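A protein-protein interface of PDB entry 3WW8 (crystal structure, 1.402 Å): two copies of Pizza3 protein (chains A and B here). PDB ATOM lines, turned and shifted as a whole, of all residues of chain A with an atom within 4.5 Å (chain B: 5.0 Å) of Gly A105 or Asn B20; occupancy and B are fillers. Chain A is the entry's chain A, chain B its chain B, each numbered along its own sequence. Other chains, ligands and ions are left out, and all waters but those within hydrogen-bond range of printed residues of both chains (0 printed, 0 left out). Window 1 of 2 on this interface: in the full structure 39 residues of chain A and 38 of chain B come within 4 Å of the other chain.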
ATOM      1  N   THR A  75     -22.647   0.498  14.839  1.00  0.00           N
ATOM      2  CA  THR A  75     -22.281  -0.186  16.069  1.00  0.00           C
ATOM      3  C   THR A  75     -22.349   0.783  17.241  1.00  0.00           C
ATOM      4  O   THR A  75     -21.876   1.930  17.160  1.00  0.00           O
ATOM      5  CB  THR A  75     -20.901  -0.846  15.979  1.00  0.00           C
ATOM      6  OG1 THR A  75     -19.944   0.121  15.532  1.00  0.00           O
ATOM      7  CG2 THR A  75     -20.931  -2.001  14.993  1.00  0.00           C
ATOM      8  N   PRO A 103     -18.914  -3.888  20.183  1.00  0.00           N
ATOM      9  CA  PRO A 103     -18.845  -4.033  18.729  1.00  0.00           C
ATOM     10  C   PRO A 103     -18.194  -2.779  18.172  1.00  0.00           C
ATOM     11  O   PRO A 103     -18.435  -1.691  18.701  1.00  0.00           O
ATOM     12  CB  PRO A 103     -20.316  -4.111  18.315  1.00  0.00           C
ATOM     13  CG  PRO A 103     -21.046  -3.373  19.392  1.00  0.00           C
ATOM     14  CD  PRO A 103     -20.289  -3.683  20.659  1.00  0.00           C
ATOM     15  N   ASN A 104     -17.351  -2.926  17.156  1.00  0.00           N
ATOM     16  CA  ASN A 104     -16.685  -1.755  16.597  1.00  0.00           C
ATOM     17  C   ASN A 104     -16.952  -1.567  15.103  1.00  0.00           C
ATOM     18  O   ASN A 104     -17.801  -0.761  14.719  1.00  0.00           O
ATOM     19  CB  ASN A 104     -15.196  -1.732  16.947  1.00  0.00           C
ATOM     20  CG  ASN A 104     -14.628  -0.327  16.930  1.00  0.00           C
ATOM     21  OD1 ASN A 104     -14.900   0.447  16.017  1.00  0.00           O
ATOM     22  ND2 ASN A 104     -13.850   0.015  17.953  1.00  0.00           N
ATOM     23  N   GLY A 105     -16.245  -2.292  14.260  1.00  0.00           N
ATOM     24  CA  GLY A 105     -16.515  -2.223  12.837  1.00  0.00           C
ATOM     25  C   GLY A 105     -17.773  -2.988  12.444  1.00  0.00           C
ATOM     26  O   GLY A 105     -18.151  -3.976  13.087  1.00  0.00           O
ATOM     27  N   VAL A 106     -18.420  -2.528  11.379  1.00  0.00           N
ATOM     28  CA  VAL A 106     -19.554  -3.223  10.785  1.00  0.00           C
ATOM     29  C   VAL A 106     -19.455  -3.187   9.253  1.00  0.00           C
ATOM     30  O   VAL A 106     -19.009  -2.189   8.658  1.00  0.00           O
ATOM     31  CB  VAL A 106     -20.914  -2.667  11.303  1.00  0.00           C
ATOM     32  CG1 VAL A 106     -21.063  -1.180  10.987  1.00  0.00           C
ATOM     33  CG2 VAL A 106     -22.092  -3.496  10.777  1.00  0.00           C
ATOM     34  N   TYR A 115     -21.779  -8.171   9.225  1.00  0.00           N
ATOM     35  CA  TYR A 115     -20.554  -8.645   9.862  1.00  0.00           C
ATOM     36  C   TYR A 115     -20.125  -7.604  10.877  1.00  0.00           C
ATOM     37  O   TYR A 115     -20.146  -6.414  10.580  1.00  0.00           O
ATOM     38  CB  TYR A 115     -19.442  -8.800   8.820  1.00  0.00           C
ATOM     39  CG  TYR A 115     -19.766  -9.743   7.687  1.00  0.00           C
ATOM     40  CD1 TYR A 115     -20.670  -9.393   6.695  1.00  0.00           C
ATOM     41  CD2 TYR A 115     -19.156 -10.987   7.606  1.00  0.00           C
ATOM     42  CE1 TYR A 115     -20.968 -10.249   5.660  1.00  0.00           C
ATOM     43  CE2 TYR A 115     -19.440 -11.851   6.567  1.00  0.00           C
ATOM     44  CZ  TYR A 115     -20.352 -11.473   5.596  1.00  0.00           C
ATOM     45  OH  TYR A 115     -20.642 -12.331   4.560  1.00  0.00           O
ATOM     46  N   VAL A 116     -19.728  -8.041  12.064  1.00  0.00           N
ATOM     47  CA  VAL A 116     -19.345  -7.122  13.125  1.00  0.00           C
ATOM     48  C   VAL A 116     -18.077  -7.591  13.827  1.00  0.00           C
ATOM     49  O   VAL A 116     -17.915  -8.780  14.132  1.00  0.00           O
ATOM     50  CB  VAL A 116     -20.484  -6.907  14.167  1.00  0.00           C
ATOM     51  CG1 VAL A 116     -20.871  -8.204  14.849  1.00  0.00           C
ATOM     52  CG2 VAL A 116     -20.087  -5.865  15.205  1.00  0.00           C
ATOM     53  N   THR A 117     -17.150  -6.665  14.037  1.00  0.00           N
ATOM     54  CA  THR A 117     -15.993  -6.951  14.848  1.00  0.00           C
ATOM     55  C   THR A 117     -16.341  -6.754  16.323  1.00  0.00           C
ATOM     56  O   THR A 117     -16.687  -5.649  16.761  1.00  0.00           O
ATOM     57  CB  THR A 117     -14.826  -6.075  14.473  1.00  0.00           C
ATOM     58  OG1 THR A 117     -14.331  -6.467  13.186  1.00  0.00           O
ATOM     59  CG2 THR A 117     -13.771  -6.272  15.452  1.00  0.00           C
ATOM     60  N   HIS A 119     -14.956  -6.383  19.444  1.00  0.00           N
ATOM     61  CA  HIS A 119     -13.643  -5.952  19.920  1.00  0.00           C
ATOM     62  C   HIS A 119     -13.290  -6.508  21.295  1.00  0.00           C
ATOM     63  O   HIS A 119     -12.177  -6.998  21.503  1.00  0.00           O
ATOM     64  CB  HIS A 119     -13.614  -4.418  19.882  1.00  0.00           C
ATOM     65  CG  HIS A 119     -12.446  -3.780  20.568  1.00  0.00           C
ATOM     66  ND1 HIS A 119     -12.422  -3.526  21.922  1.00  0.00           N
ATOM     67  CD2 HIS A 119     -11.312  -3.243  20.063  1.00  0.00           C
ATOM     68  CE1 HIS A 119     -11.293  -2.910  22.231  1.00  0.00           C
ATOM     69  NE2 HIS A 119     -10.604  -2.719  21.123  1.00  0.00           N
ATOM     70  N   THR B  18      -8.126  -7.206  20.162  1.00  0.00           N
ATOM     71  CA  THR B  18      -8.799  -5.921  19.941  1.00  0.00           C
ATOM     72  C   THR B  18      -9.082  -5.614  18.472  1.00  0.00           C
ATOM     73  O   THR B  18      -8.752  -4.523  17.992  1.00  0.00           O
ATOM     74  CB  THR B  18      -8.041  -4.752  20.602  1.00  0.00           C
ATOM     75  OG1 THR B  18      -6.686  -4.715  20.135  1.00  0.00           O
ATOM     76  CG2 THR B  18      -8.051  -4.899  22.121  1.00  0.00           C
ATOM     77  N   PRO B  19      -9.705  -6.570  17.756  1.00  0.00           N
ATOM     78  CA  PRO B  19      -9.980  -6.283  16.343  1.00  0.00           C
ATOM     79  C   PRO B  19     -10.944  -5.108  16.254  1.00  0.00           C
ATOM     80  O   PRO B  19     -11.749  -4.915  17.166  1.00  0.00           O
ATOM     81  CB  PRO B  19     -10.621  -7.581  15.844  1.00  0.00           C
ATOM     82  CG  PRO B  19     -11.232  -8.209  17.073  1.00  0.00           C
ATOM     83  CD  PRO B  19     -10.338  -7.825  18.215  1.00  0.00           C
ATOM     84  N   ASN B  20     -10.877  -4.312  15.196  1.00  0.00           N
ATOM     85  CA  ASN B  20     -11.707  -3.098  15.205  1.00  0.00           C
ATOM     86  C   ASN B  20     -12.187  -2.547  13.872  1.00  0.00           C
ATOM     87  O   ASN B  20     -12.630  -1.388  13.792  1.00  0.00           O
ATOM     88  CB  ASN B  20     -11.005  -1.995  15.985  1.00  0.00           C
ATOM     89  CG  ASN B  20      -9.676  -1.664  15.403  1.00  0.00           C
ATOM     90  OD1 ASN B  20      -9.341  -2.133  14.312  1.00  0.00           O
ATOM     91  ND2 ASN B  20      -8.885  -0.868  16.120  1.00  0.00           N
ATOM     92  N   GLY B  21     -12.092  -3.349  12.826  1.00  0.00           N
ATOM     93  CA  GLY B  21     -12.571  -2.947  11.515  1.00  0.00           C
ATOM     94  C   GLY B  21     -12.838  -4.198  10.714  1.00  0.00           C
ATOM     95  O   GLY B  21     -12.086  -5.171  10.838  1.00  0.00           O
ATOM     96  N   VAL B  22     -13.897  -4.181   9.909  1.00  0.00           N
ATOM     97  CA  VAL B  22     -14.261  -5.320   9.073  1.00  0.00           C
ATOM     98  C   VAL B  22     -14.790  -4.848   7.717  1.00  0.00           C
ATOM     99  O   VAL B  22     -15.441  -3.798   7.614  1.00  0.00           O
ATOM    100  CB  VAL B  22     -15.267  -6.259   9.786  1.00  0.00           C
ATOM    101  CG1 VAL B  22     -16.595  -5.547  10.035  1.00  0.00           C
ATOM    102  CG2 VAL B  22     -15.481  -7.541   8.982  1.00  0.00           C
ATOM    103  N   THR B  33      -9.175  -5.794  10.492  1.00  0.00           N
ATOM    104  CA  THR B  33      -8.002  -5.182  11.108  1.00  0.00           C
ATOM    105  C   THR B  33      -7.800  -5.746  12.504  1.00  0.00           C
ATOM    106  O   THR B  33      -8.546  -5.450  13.443  1.00  0.00           O
ATOM    107  CB  THR B  33      -8.071  -3.637  11.120  1.00  0.00           C
ATOM    108  OG1 THR B  33      -9.331  -3.198  11.639  1.00  0.00           O
ATOM    109  CG2 THR B  33      -7.915  -3.109   9.713  1.00  0.00           C
ATOM    110  N   HIS B  35      -6.132  -5.220  15.148  1.00  0.00           N
ATOM    111  CA  HIS B  35      -5.436  -4.046  15.671  1.00  0.00           C
ATOM    112  C   HIS B  35      -4.332  -4.371  16.678  1.00  0.00           C
ATOM    113  O   HIS B  35      -3.213  -3.878  16.551  1.00  0.00           O
ATOM    114  CB  HIS B  35      -6.512  -3.095  16.235  1.00  0.00           C
ATOM    115  CG  HIS B  35      -6.021  -2.092  17.233  1.00  0.00           C
ATOM    116  ND1 HIS B  35      -5.976  -2.357  18.586  1.00  0.00           N
ATOM    117  CD2 HIS B  35      -5.652  -0.802  17.090  1.00  0.00           C
ATOM    118  CE1 HIS B  35      -5.538  -1.288  19.224  1.00  0.00           C
ATOM    119  NE2 HIS B  35      -5.346  -0.323  18.343  1.00  0.00           N
ATOM    120  N   PRO B  61      -3.424  -0.619  13.339  1.00  0.00           N
ATOM    121  CA  PRO B  61      -4.374  -0.312  12.262  1.00  0.00           C
ATOM    122  C   PRO B  61      -5.791  -0.394  12.782  1.00  0.00           C
ATOM    123  O   PRO B  61      -6.077  -1.142  13.722  1.00  0.00           O
ATOM    124  CB  PRO B  61      -4.124  -1.421  11.238  1.00  0.00           C
ATOM    125  CG  PRO B  61      -3.565  -2.565  12.047  1.00  0.00           C
ATOM    126  CD  PRO B  61      -2.766  -1.927  13.146  1.00  0.00           C
ATOM    127  N   ASN B  62      -6.673   0.412  12.209  1.00  0.00           N
ATOM    128  CA  ASN B  62      -8.052   0.366  12.643  1.00  0.00           C
ATOM    129  C   ASN B  62      -9.080   0.185  11.509  1.00  0.00           C
ATOM    130  O   ASN B  62      -9.700  -0.883  11.424  1.00  0.00           O
ATOM    131  CB  ASN B  62      -8.370   1.480  13.658  1.00  0.00           C
ATOM    132  CG  ASN B  62      -7.921   2.852  13.202  1.00  0.00           C
ATOM    133  OD1 ASN B  62      -7.641   3.066  12.030  1.00  0.00           O
ATOM    134  ND2 ASN B  62      -7.883   3.804  14.139  1.00  0.00           N
ATOM    135  N   GLY B  63      -9.233   1.153  10.624  1.00  0.00           N
ATOM    136  CA  GLY B  63     -10.234   1.024   9.579  1.00  0.00           C
ATOM    137  C   GLY B  63      -9.810   0.125   8.428  1.00  0.00           C
ATOM    138  O   GLY B  63      -8.626   0.037   8.091  1.00  0.00           O
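O of Gly B21 is in hydrogen-bond range of OG1 of Thr A117 (3.5 Å).
The backbone carbonyl oxygen (O) of Asn A104 lies within hydrogen-bond range of the side-chain hydroxyl (OG1) of Thr A75 (2.5 Å).
The backbone NH (N) of Asn A104 is in hydrogen-bond range of the backbone carbonyl oxygen (O) of Thr A117 (2.8 Å).
N of Thr A117 lies within hydrogen-bond range of O of Gly A105 (3.0 Å).
The side-chain hydroxyl (OG1) of Thr B33 is in hydrogen-bond range of the side-chain amide oxygen (OD1) of Asn B20, at 2.9 Å.
The side-chain amide oxygen of Asn B20 lies close to the backbone carbonyl oxygen of Pro B61 (3.5 Å).
OD1 of Asn B20 lies close to O of Asn B62, 3.2 Å away.
Among the printed residues, pairs that only touch across the chains: Thr A117 with Pro B19, His A119 with Thr B18, His A119 with Pro B19, Thr A117 with Asn B20, Thr A117 with Val B22, Asn A104 with Asn B20, Tyr A115 with Val B22, Gly A105 with Val B22, Gly A105 with Asn B20 and Val A106 with Val B22.
Of the printed residues of chain B, Asn A104 touches Asn B20.
Gly A105 touches just these residues of chain B: Asn B20 (3.8 Å) and Val B22 (3.7 Å).
Printed residues of chain B within 4 Å of Tyr A115: Val B22 (3.7 Å).
Val A116 touches none of the printed residues of chain B.
Of the printed residues of chain A, Thr B18 touches His A119 (3.3 Å).
Of chain A, only Asn A104 (3.7 Å), Gly A105 (3.8 Å) and Thr A117 (3.5 Å) come within 4 Å of Asn B20.
Gly B63 touches none of the printed residues of chain A.
The nearest residue of chain A that does not touch Asn B20 is His A119 (4.3 Å).
Hydrophobic or aromatic side chains of chain B within 4 Å of the printed part of chain A: Pro B19 and Val B22.
Of the 9 printed residues of chain A, 6 touch a printed residue of chain B.
Printed residues of chain A that touch a printed residue of chain B: Asn A104, Gly A105, Val A106, Tyr A115, Thr A117 and His A119.
Among the printed residues, no Asp or Glu carboxylate lies within 4 Å of a Lys or Arg side-chain nitrogen of the other chain.
No position is printed for both chains.
Of the 11 pairs that touch across the chains among the printed residues, none has its exchanged pair printed and touching as well.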
